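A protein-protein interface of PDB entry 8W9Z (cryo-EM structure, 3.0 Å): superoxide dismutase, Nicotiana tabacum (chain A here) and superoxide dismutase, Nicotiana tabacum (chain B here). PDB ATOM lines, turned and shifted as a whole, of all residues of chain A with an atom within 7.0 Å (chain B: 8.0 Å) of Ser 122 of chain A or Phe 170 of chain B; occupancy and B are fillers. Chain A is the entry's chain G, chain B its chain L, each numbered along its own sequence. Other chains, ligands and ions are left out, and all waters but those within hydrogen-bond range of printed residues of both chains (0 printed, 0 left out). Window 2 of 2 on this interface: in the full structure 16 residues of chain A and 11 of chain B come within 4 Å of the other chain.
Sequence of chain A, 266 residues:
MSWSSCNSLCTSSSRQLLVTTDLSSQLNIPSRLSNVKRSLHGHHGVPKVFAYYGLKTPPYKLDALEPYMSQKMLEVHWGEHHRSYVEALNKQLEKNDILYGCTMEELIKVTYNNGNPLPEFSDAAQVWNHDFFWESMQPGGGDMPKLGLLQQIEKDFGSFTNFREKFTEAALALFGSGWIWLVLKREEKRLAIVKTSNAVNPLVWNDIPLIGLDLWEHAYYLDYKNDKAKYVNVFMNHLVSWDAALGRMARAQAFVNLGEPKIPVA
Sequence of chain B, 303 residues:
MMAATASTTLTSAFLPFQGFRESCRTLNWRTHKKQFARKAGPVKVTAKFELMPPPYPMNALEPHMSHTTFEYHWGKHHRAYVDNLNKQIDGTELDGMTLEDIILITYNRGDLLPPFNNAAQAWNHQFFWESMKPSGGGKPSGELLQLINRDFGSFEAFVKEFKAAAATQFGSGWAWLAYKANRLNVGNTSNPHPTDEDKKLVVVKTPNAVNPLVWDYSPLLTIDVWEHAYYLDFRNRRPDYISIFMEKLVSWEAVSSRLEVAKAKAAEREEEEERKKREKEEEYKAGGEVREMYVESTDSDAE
N of Asn 208 of chain B sits at hydrogen-bond distance from O of Ser 172 of chain B (3.0 Å).
The side-chain amide oxygen (OE1) of Gln 126 of chain A lies close to the backbone carbonyl oxygen (O) of Asn 198 of chain A.
The side-chain amide nitrogen (ND2) of Asn 129 of chain A lies within hydrogen-bond range of the backbone carbonyl oxygen (O) of Ala 199 of chain A, 3.1 Å away.
The backbone carbonyl oxygen of Ser 177 of chain A sits close to the side-chain amide oxygen of Asn 198 of chain A (3.1 Å).
NE1 of Trp 216 of chain A lies within hydrogen-bond range of O of Asn 198 of chain A, 2.8 Å away.
Tyr 85 of chain A touches Phe 170 of chain B.
CZ of Phe 170 of chain B touches CB of Ser 122 of chain A, at 3.97 Å.
Ser 172 of chain B touches Ser 177 of chain A (N to OG, 3.95 Å).
ND2 of Asn 198 of chain A touches O of Phe 170 of chain B (3.7 Å).
Phe 170 of chain B touches Ala 199 of chain A (CE2 to CB, 3.8 Å).
Phe 170 of chain B touches Trp 216 of chain A (CZ to CH2, 3.6 Å).
Trp 216 of chain A touches Gly 171 of chain B.
Of the printed residues of chain B, Tyr 85 of chain A touches Phe 170 (3.98 Å).
Printed residues of chain B within 4 Å of Asn 198 of chain A: Phe 170.
Of the printed residues of chain B, Ala 199 of chain A touches Phe 170.
Ala 165 of chain B touches none of the printed residues of chain A.
Of the printed residues of chain A, Gly 171 of chain B touches Trp 216.
Of the printed residues of chain A, Ser 172 of chain B touches Ser 177.
Pro 207 of chain B touches none of the printed residues of chain A.
The nearest printed residue of chain A that does not touch Phe 170 of chain B is Gln 126 of chain A (4.1 Å).
Of the 20 printed residues of chain A, 6 touch a printed residue of chain B.
Hydrophobic or aromatic side chains of chain B within 4 Å of the printed part of chain A: Phe 170.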
ATOM      1  N   TYR A  85      12.041  -4.342 -15.022  1.00  0.00           N
ATOM      2  CA  TYR A  85      11.902  -3.473 -16.143  1.00  0.00           C
ATOM      3  C   TYR A  85      13.247  -3.306 -16.780  1.00  0.00           C
ATOM      4  O   TYR A  85      13.377  -3.422 -17.983  1.00  0.00           O
ATOM      5  CB  TYR A  85      11.380  -2.134 -15.691  1.00  0.00           C
ATOM      6  CG  TYR A  85       9.891  -2.075 -15.514  1.00  0.00           C
ATOM      7  CD1 TYR A  85       9.041  -2.361 -16.565  1.00  0.00           C
ATOM      8  CD2 TYR A  85       9.332  -1.706 -14.305  1.00  0.00           C
ATOM      9  CE1 TYR A  85       7.674  -2.299 -16.414  1.00  0.00           C
ATOM     10  CE2 TYR A  85       7.966  -1.644 -14.143  1.00  0.00           C
ATOM     11  CZ  TYR A  85       7.143  -1.941 -15.204  1.00  0.00           C
ATOM     12  OH  TYR A  85       5.783  -1.880 -15.057  1.00  0.00           O
ATOM     13  N   GLN A  92      15.743  -5.664 -24.951  1.00  0.00           N
ATOM     14  CA  GLN A  92      15.231  -5.013 -26.151  1.00  0.00           C
ATOM     15  C   GLN A  92      16.274  -4.121 -26.814  1.00  0.00           C
ATOM     16  O   GLN A  92      16.261  -3.972 -28.041  1.00  0.00           O
ATOM     17  CB  GLN A  92      13.978  -4.201 -25.817  1.00  0.00           C
ATOM     18  CG  GLN A  92      12.748  -5.052 -25.547  1.00  0.00           C
ATOM     19  CD  GLN A  92      11.558  -4.233 -25.089  1.00  0.00           C
ATOM     20  OE1 GLN A  92      10.416  -4.522 -25.447  1.00  0.00           O
ATOM     21  NE2 GLN A  92      11.818  -3.209 -24.288  1.00  0.00           N
ATOM     22  N   THR A 111      10.924   6.650 -29.021  1.00  0.00           N
ATOM     23  CA  THR A 111      10.087   5.462 -28.931  1.00  0.00           C
ATOM     24  C   THR A 111       8.611   5.791 -28.762  1.00  0.00           C
ATOM     25  O   THR A 111       7.767   4.922 -29.008  1.00  0.00           O
ATOM     26  CB  THR A 111      10.544   4.573 -27.772  1.00  0.00           C
ATOM     27  OG1 THR A 111      10.614   5.349 -26.569  1.00  0.00           O
ATOM     28  CG2 THR A 111      11.909   3.975 -28.067  1.00  0.00           C
ATOM     29  N   PRO A 117       3.348   4.259 -30.108  1.00  0.00           N
ATOM     30  CA  PRO A 117       4.592   3.895 -29.420  1.00  0.00           C
ATOM     31  C   PRO A 117       5.206   2.612 -29.957  1.00  0.00           C
ATOM     32  O   PRO A 117       4.512   1.678 -30.362  1.00  0.00           O
ATOM     33  CB  PRO A 117       4.152   3.724 -27.960  1.00  0.00           C
ATOM     34  CG  PRO A 117       2.840   4.435 -27.860  1.00  0.00           C
ATOM     35  CD  PRO A 117       2.197   4.258 -29.194  1.00  0.00           C
ATOM     36  N   LEU A 118       6.537   2.585 -29.952  1.00  0.00           N
ATOM     37  CA  LEU A 118       7.279   1.387 -30.296  1.00  0.00           C
ATOM     38  C   LEU A 118       7.179   0.370 -29.160  1.00  0.00           C
ATOM     39  O   LEU A 118       6.841   0.725 -28.028  1.00  0.00           O
ATOM     40  CB  LEU A 118       8.737   1.741 -30.581  1.00  0.00           C
ATOM     41  CG  LEU A 118       8.976   2.672 -31.772  1.00  0.00           C
ATOM     42  CD1 LEU A 118      10.463   2.839 -32.033  1.00  0.00           C
ATOM     43  CD2 LEU A 118       8.265   2.152 -33.008  1.00  0.00           C
ATOM     44  N   PRO A 119       7.463  -0.908 -29.435  1.00  0.00           N
ATOM     45  CA  PRO A 119       7.285  -1.938 -28.398  1.00  0.00           C
ATOM     46  C   PRO A 119       8.205  -1.792 -27.196  1.00  0.00           C
ATOM     47  O   PRO A 119       8.013  -2.518 -26.212  1.00  0.00           O
ATOM     48  CB  PRO A 119       7.564  -3.247 -29.149  1.00  0.00           C
ATOM     49  CG  PRO A 119       8.381  -2.842 -30.325  1.00  0.00           C
ATOM     50  CD  PRO A 119       7.853  -1.503 -30.725  1.00  0.00           C
ATOM     51  N   GLU A 120       9.188  -0.894 -27.232  1.00  0.00           N
ATOM     52  CA  GLU A 120      10.095  -0.700 -26.109  1.00  0.00           C
ATOM     53  C   GLU A 120       9.891   0.638 -25.412  1.00  0.00           C
ATOM     54  O   GLU A 120      10.681   0.994 -24.532  1.00  0.00           O
ATOM     55  CB  GLU A 120      11.549  -0.833 -26.570  1.00  0.00           C
ATOM     56  CG  GLU A 120      12.071   0.358 -27.351  1.00  0.00           C
ATOM     57  CD  GLU A 120      13.568   0.286 -27.579  1.00  0.00           C
ATOM     58  OE1 GLU A 120      14.071  -0.811 -27.898  1.00  0.00           O
ATOM     59  OE2 GLU A 120      14.244   1.326 -27.425  1.00  0.00           O
ATOM     60  N   PHE A 121       8.849   1.386 -25.779  1.00  0.00           N
ATOM     61  CA  PHE A 121       8.608   2.677 -25.142  1.00  0.00           C
ATOM     62  C   PHE A 121       8.173   2.506 -23.694  1.00  0.00           C
ATOM     63  O   PHE A 121       8.669   3.202 -22.800  1.00  0.00           O
ATOM     64  CB  PHE A 121       7.558   3.466 -25.918  1.00  0.00           C
ATOM     65  CG  PHE A 121       6.981   4.617 -25.146  1.00  0.00           C
ATOM     66  CD1 PHE A 121       7.705   5.783 -24.973  1.00  0.00           C
ATOM     67  CD2 PHE A 121       5.717   4.531 -24.588  1.00  0.00           C
ATOM     68  CE1 PHE A 121       7.179   6.842 -24.259  1.00  0.00           C
ATOM     69  CE2 PHE A 121       5.187   5.587 -23.876  1.00  0.00           C
ATOM     70  CZ  PHE A 121       5.918   6.743 -23.711  1.00  0.00           C
ATOM     71  N   SER A 122       7.228   1.594 -23.449  1.00  0.00           N
ATOM     72  CA  SER A 122       6.678   1.433 -22.108  1.00  0.00           C
ATOM     73  C   SER A 122       7.762   1.072 -21.102  1.00  0.00           C
ATOM     74  O   SER A 122       7.790   1.609 -19.990  1.00  0.00           O
ATOM     75  CB  SER A 122       5.581   0.370 -22.118  1.00  0.00           C
ATOM     76  OG  SER A 122       6.086  -0.876 -22.564  1.00  0.00           O
ATOM     77  N   ASP A 123       8.684   0.191 -21.488  1.00  0.00           N
ATOM     78  CA  ASP A 123       9.692  -0.285 -20.548  1.00  0.00           C
ATOM     79  C   ASP A 123      10.674   0.819 -20.172  1.00  0.00           C
ATOM     80  O   ASP A 123      10.942   1.047 -18.986  1.00  0.00           O
ATOM     81  CB  ASP A 123      10.428  -1.481 -21.141  1.00  0.00           C
ATOM     82  CG  ASP A 123      11.211  -2.241 -20.105  1.00  0.00           C
ATOM     83  OD1 ASP A 123      11.084  -1.911 -18.909  1.00  0.00           O
ATOM     84  OD2 ASP A 123      11.951  -3.168 -20.484  1.00  0.00           O
ATOM     85  N   ALA A 124      11.241   1.500 -21.171  1.00  0.00           N
ATOM     86  CA  ALA A 124      12.175   2.584 -20.884  1.00  0.00           C
ATOM     87  C   ALA A 124      11.488   3.713 -20.128  1.00  0.00           C
ATOM     88  O   ALA A 124      12.077   4.315 -19.219  1.00  0.00           O
ATOM     89  CB  ALA A 124      12.791   3.104 -22.182  1.00  0.00           C
ATOM     90  N   ALA A 125      10.254   3.990 -20.474  1.00  0.00           N
ATOM     91  CA  ALA A 125       9.584   5.026 -19.765  1.00  0.00           C
ATOM     92  C   ALA A 125       9.502   4.595 -18.336  1.00  0.00           C
ATOM     93  O   ALA A 125       9.706   5.388 -17.449  1.00  0.00           O
ATOM     94  CB  ALA A 125       8.228   5.275 -20.331  1.00  0.00           C
ATOM     95  N   GLN A 126       9.206   3.342 -18.082  1.00  0.00           N
ATOM     96  CA  GLN A 126       9.050   2.956 -16.705  1.00  0.00           C
ATOM     97  C   GLN A 126      10.341   3.086 -15.955  1.00  0.00           C
ATOM     98  O   GLN A 126      10.342   3.483 -14.806  1.00  0.00           O
ATOM     99  CB  GLN A 126       8.458   1.573 -16.551  1.00  0.00           C
ATOM    100  CG  GLN A 126       6.959   1.525 -16.785  1.00  0.00           C
ATOM    101  CD  GLN A 126       6.184   2.264 -15.716  1.00  0.00           C
ATOM    102  OE1 GLN A 126       5.525   3.264 -15.988  1.00  0.00           O
ATOM    103  NE2 GLN A 126       6.262   1.775 -14.491  1.00  0.00           N
ATOM    104  N   VAL A 127      11.447   2.727 -16.580  1.00  0.00           N
ATOM    105  CA  VAL A 127      12.688   2.770 -15.857  1.00  0.00           C
ATOM    106  C   VAL A 127      12.981   4.195 -15.464  1.00  0.00           C
ATOM    107  O   VAL A 127      13.295   4.480 -14.318  1.00  0.00           O
ATOM    108  CB  VAL A 127      13.834   2.246 -16.695  1.00  0.00           C
ATOM    109  CG1 VAL A 127      15.144   2.384 -15.948  1.00  0.00           C
ATOM    110  CG2 VAL A 127      13.593   0.795 -17.050  1.00  0.00           C
ATOM    111  N   ASN A 129      10.859   6.554 -15.230  1.00  0.00           N
ATOM    112  CA  ASN A 129       9.845   7.018 -14.323  1.00  0.00           C
ATOM    113  C   ASN A 129      10.183   6.600 -12.931  1.00  0.00           C
ATOM    114  O   ASN A 129      10.135   7.395 -12.011  1.00  0.00           O
ATOM    115  CB  ASN A 129       8.501   6.477 -14.733  1.00  0.00           C
ATOM    116  CG  ASN A 129       7.875   7.268 -15.843  1.00  0.00           C
ATOM    117  OD1 ASN A 129       8.328   8.354 -16.166  1.00  0.00           O
ATOM    118  ND2 ASN A 129       6.823   6.728 -16.432  1.00  0.00           N
ATOM    119  N   SER A 177      -4.066   2.561 -13.550  1.00  0.00           N
ATOM    120  CA  SER A 177      -2.695   2.839 -13.199  1.00  0.00           C
ATOM    121  C   SER A 177      -2.210   4.055 -13.947  1.00  0.00           C
ATOM    122  O   SER A 177      -2.753   4.390 -14.989  1.00  0.00           O
ATOM    123  CB  SER A 177      -1.861   1.646 -13.578  1.00  0.00           C
ATOM    124  OG  SER A 177      -2.377   0.473 -12.980  1.00  0.00           O
ATOM    125  N   ASN A 198      -0.543   4.919 -18.153  1.00  0.00           N
ATOM    126  CA  ASN A 198       0.234   3.894 -17.462  1.00  0.00           C
ATOM    127  C   ASN A 198       1.718   4.245 -17.393  1.00  0.00           C
ATOM    128  O   ASN A 198       2.297   4.341 -16.305  1.00  0.00           O
ATOM    129  CB  ASN A 198       0.035   2.547 -18.156  1.00  0.00           C
ATOM    130  CG  ASN A 198      -1.425   2.161 -18.270  1.00  0.00           C
ATOM    131  OD1 ASN A 198      -2.245   2.540 -17.436  1.00  0.00           O
ATOM    132  ND2 ASN A 198      -1.756   1.402 -19.308  1.00  0.00           N
ATOM    133  N   ALA A 199       2.353   4.438 -18.548  1.00  0.00           N
ATOM    134  CA  ALA A 199       3.791   4.653 -18.601  1.00  0.00           C
ATOM    135  C   ALA A 199       4.209   5.971 -19.235  1.00  0.00           C
ATOM    136  O   ALA A 199       5.400   6.299 -19.195  1.00  0.00           O
ATOM    137  CB  ALA A 199       4.476   3.504 -19.360  1.00  0.00           C
ATOM    138  N   VAL A 200       3.281   6.732 -19.813  1.00  0.00           N
ATOM    139  CA  VAL A 200       3.644   7.973 -20.485  1.00  0.00           C
ATOM    140  C   VAL A 200       4.129   8.987 -19.458  1.00  0.00           C
ATOM    141  O   VAL A 200       3.507   9.179 -18.406  1.00  0.00           O
ATOM    142  CB  VAL A 200       2.454   8.515 -21.292  1.00  0.00           C
ATOM    143  CG1 VAL A 200       2.731   9.929 -21.769  1.00  0.00           C
ATOM    144  CG2 VAL A 200       2.170   7.606 -22.477  1.00  0.00           C
ATOM    145  N   TRP A 216       0.239   3.568  -9.705  1.00  0.00           N
ATOM    146  CA  TRP A 216       0.042   2.168  -9.998  1.00  0.00           C
ATOM    147  C   TRP A 216      -0.163   1.494  -8.677  1.00  0.00           C
ATOM    148  O   TRP A 216       0.480   1.833  -7.696  1.00  0.00           O
ATOM    149  CB  TRP A 216       1.264   1.563 -10.660  1.00  0.00           C
ATOM    150  CG  TRP A 216       1.421   1.851 -12.096  1.00  0.00           C
ATOM    151  CD1 TRP A 216       1.455   3.069 -12.687  1.00  0.00           C
ATOM    152  CD2 TRP A 216       1.605   0.893 -13.136  1.00  0.00           C
ATOM    153  NE1 TRP A 216       1.626   2.934 -14.035  1.00  0.00           N
ATOM    154  CE2 TRP A 216       1.725   1.604 -14.336  1.00  0.00           C
ATOM    155  CE3 TRP A 216       1.664  -0.499 -13.168  1.00  0.00           C
ATOM    156  CZ2 TRP A 216       1.906   0.972 -15.555  1.00  0.00           C
ATOM    157  CZ3 TRP A 216       1.846  -1.123 -14.376  1.00  0.00           C
ATOM    158  CH2 TRP A 216       1.963  -0.390 -15.553  1.00  0.00           C
ATOM    159  N   ALA B 165      -2.016 -13.906 -23.788  1.00  0.00           N
ATOM    160  CA  ALA B 165      -2.643 -12.614 -23.919  1.00  0.00           C
ATOM    161  C   ALA B 165      -2.753 -11.947 -22.581  1.00  0.00           C
ATOM    162  O   ALA B 165      -2.561 -10.748 -22.458  1.00  0.00           O
ATOM    163  CB  ALA B 165      -4.002 -12.745 -24.546  1.00  0.00           C
ATOM    164  N   ALA B 166      -3.083 -12.723 -21.572  1.00  0.00           N
ATOM    165  CA  ALA B 166      -3.233 -12.153 -20.264  1.00  0.00           C
ATOM    166  C   ALA B 166      -1.923 -11.594 -19.791  1.00  0.00           C
ATOM    167  O   ALA B 166      -1.877 -10.515 -19.216  1.00  0.00           O
ATOM    168  CB  ALA B 166      -3.706 -13.202 -19.308  1.00  0.00           C
ATOM    169  N   ALA B 167      -0.842 -12.316 -20.032  1.00  0.00           N
ATOM    170  CA  ALA B 167       0.448 -11.869 -19.543  1.00  0.00           C
ATOM    171  C   ALA B 167       0.856 -10.556 -20.160  1.00  0.00           C
ATOM    172  O   ALA B 167       1.386  -9.684 -19.489  1.00  0.00           O
ATOM    173  CB  ALA B 167       1.498 -12.914 -19.833  1.00  0.00           C
ATOM    174  N   THR B 168       0.598 -10.403 -21.444  1.00  0.00           N
ATOM    175  CA  THR B 168       1.032  -9.208 -22.134  1.00  0.00           C
ATOM    176  C   THR B 168       0.201  -7.970 -21.894  1.00  0.00           C
ATOM    177  O   THR B 168       0.555  -6.900 -22.364  1.00  0.00           O
ATOM    178  CB  THR B 168       1.057  -9.442 -23.641  1.00  0.00           C
ATOM    179  OG1 THR B 168      -0.252  -9.812 -24.085  1.00  0.00           O
ATOM    180  CG2 THR B 168       2.036 -10.546 -23.986  1.00  0.00           C
ATOM    181  N   GLN B 169      -0.905  -8.083 -21.184  1.00  0.00           N
ATOM    182  CA  GLN B 169      -1.640  -6.871 -20.907  1.00  0.00           C
ATOM    183  C   GLN B 169      -0.769  -6.013 -20.037  1.00  0.00           C
ATOM    184  O   GLN B 169      -0.167  -6.500 -19.085  1.00  0.00           O
ATOM    185  CB  GLN B 169      -2.977  -7.150 -20.237  1.00  0.00           C
ATOM    186  CG  GLN B 169      -3.736  -5.915 -19.788  1.00  0.00           C
ATOM    187  CD  GLN B 169      -4.203  -5.055 -20.941  1.00  0.00           C
ATOM    188  OE1 GLN B 169      -4.334  -5.523 -22.069  1.00  0.00           O
ATOM    189  NE2 GLN B 169      -4.473  -3.790 -20.657  1.00  0.00           N
ATOM    190  N   PHE B 170      -0.710  -4.726 -20.349  1.00  0.00           N
ATOM    191  CA  PHE B 170       0.118  -3.818 -19.591  1.00  0.00           C
ATOM    192  C   PHE B 170      -0.816  -2.922 -18.827  1.00  0.00           C
ATOM    193  O   PHE B 170      -1.712  -2.318 -19.401  1.00  0.00           O
ATOM    194  CB  PHE B 170       0.962  -2.992 -20.551  1.00  0.00           C
ATOM    195  CG  PHE B 170       1.974  -2.118 -19.879  1.00  0.00           C
ATOM    196  CD1 PHE B 170       3.059  -2.670 -19.230  1.00  0.00           C
ATOM    197  CD2 PHE B 170       1.851  -0.743 -19.918  1.00  0.00           C
ATOM    198  CE1 PHE B 170       3.994  -1.868 -18.614  1.00  0.00           C
ATOM    199  CE2 PHE B 170       2.783   0.065 -19.306  1.00  0.00           C
ATOM    200  CZ  PHE B 170       3.856  -0.498 -18.654  1.00  0.00           C
ATOM    201  N   GLY B 171      -0.612  -2.830 -17.527  1.00  0.00           N
ATOM    202  CA  GLY B 171      -1.464  -1.993 -16.719  1.00  0.00           C
ATOM    203  C   GLY B 171      -2.730  -2.709 -16.334  1.00  0.00           C
ATOM    204  O   GLY B 171      -2.836  -3.917 -16.496  1.00  0.00           O
ATOM    205  N   SER B 172      -3.686  -1.976 -15.795  1.00  0.00           N
ATOM    206  CA  SER B 172      -4.939  -2.575 -15.425  1.00  0.00           C
ATOM    207  C   SER B 172      -5.702  -3.015 -16.653  1.00  0.00           C
ATOM    208  O   SER B 172      -5.723  -2.315 -17.657  1.00  0.00           O
ATOM    209  CB  SER B 172      -5.760  -1.583 -14.629  1.00  0.00           C
ATOM    210  OG  SER B 172      -7.043  -2.108 -14.324  1.00  0.00           O
ATOM    211  N   GLY B 173      -6.315  -4.191 -16.582  1.00  0.00           N
ATOM    212  CA  GLY B 173      -7.048  -4.706 -17.717  1.00  0.00           C
ATOM    213  C   GLY B 173      -7.830  -5.959 -17.435  1.00  0.00           C
ATOM    214  O   GLY B 173      -7.796  -6.464 -16.319  1.00  0.00           O
ATOM    215  N   LYS B 205      -7.911  -8.699 -25.483  1.00  0.00           N
ATOM    216  CA  LYS B 205      -7.365  -8.059 -24.302  1.00  0.00           C
ATOM    217  C   LYS B 205      -8.017  -6.712 -24.199  1.00  0.00           C
ATOM    218  O   LYS B 205      -8.198  -6.032 -25.198  1.00  0.00           O
ATOM    219  CB  LYS B 205      -5.865  -7.878 -24.441  1.00  0.00           C
ATOM    220  N   THR B 206      -8.307  -6.288 -22.986  1.00  0.00           N
ATOM    221  CA  THR B 206      -8.907  -4.992 -22.821  1.00  0.00           C
ATOM    222  C   THR B 206      -8.201  -4.071 -21.837  1.00  0.00           C
ATOM    223  O   THR B 206      -7.616  -4.524 -20.860  1.00  0.00           O
ATOM    224  CB  THR B 206     -10.388  -5.141 -22.479  1.00  0.00           C
ATOM    225  OG1 THR B 206     -11.086  -3.953 -22.853  1.00  0.00           O
ATOM    226  CG2 THR B 206     -10.578  -5.412 -21.011  1.00  0.00           C
ATOM    227  N   PRO B 207      -8.229  -2.765 -22.104  1.00  0.00           N
ATOM    228  CA  PRO B 207      -7.633  -1.792 -21.199  1.00  0.00           C
ATOM    229  C   PRO B 207      -8.502  -1.666 -20.000  1.00  0.00           C
ATOM    230  O   PRO B 207      -9.556  -2.273 -19.961  1.00  0.00           O
ATOM    231  CB  PRO B 207      -7.729  -0.515 -21.990  1.00  0.00           C
ATOM    232  CG  PRO B 207      -7.562  -0.959 -23.386  1.00  0.00           C
ATOM    233  CD  PRO B 207      -8.349  -2.227 -23.467  1.00  0.00           C
ATOM    234  N   ASN B 208      -8.082  -0.926 -18.997  1.00  0.00           N
ATOM    235  CA  ASN B 208      -8.872  -0.882 -17.791  1.00  0.00           C
ATOM    236  C   ASN B 208     -10.292  -0.454 -18.047  1.00  0.00           C
ATOM    237  O   ASN B 208     -10.528   0.522 -18.745  1.00  0.00           O
ATOM    238  CB  ASN B 208      -8.251   0.091 -16.805  1.00  0.00           C
ATOM    239  CG  ASN B 208      -7.563   1.271 -17.477  1.00  0.00           C
ATOM    240  OD1 ASN B 208      -8.011   1.778 -18.503  1.00  0.00           O
ATOM    241  ND2 ASN B 208      -6.472   1.725 -16.876  1.00  0.00           N
ATOM    242  N   VAL B 225      -7.045  -8.852 -14.557  1.00  0.00           N
ATOM    243  CA  VAL B 225      -5.597  -8.726 -14.532  1.00  0.00           C
ATOM    244  C   VAL B 225      -5.248  -7.455 -13.820  1.00  0.00           C
ATOM    245  O   VAL B 225      -4.083  -7.175 -13.579  1.00  0.00           O
ATOM    246  CB  VAL B 225      -4.943  -8.821 -15.918  1.00  0.00           C
ATOM    247  CG1 VAL B 225      -5.674  -9.828 -16.785  1.00  0.00           C
ATOM    248  CG2 VAL B 225      -4.879  -7.473 -16.606  1.00  0.00           C
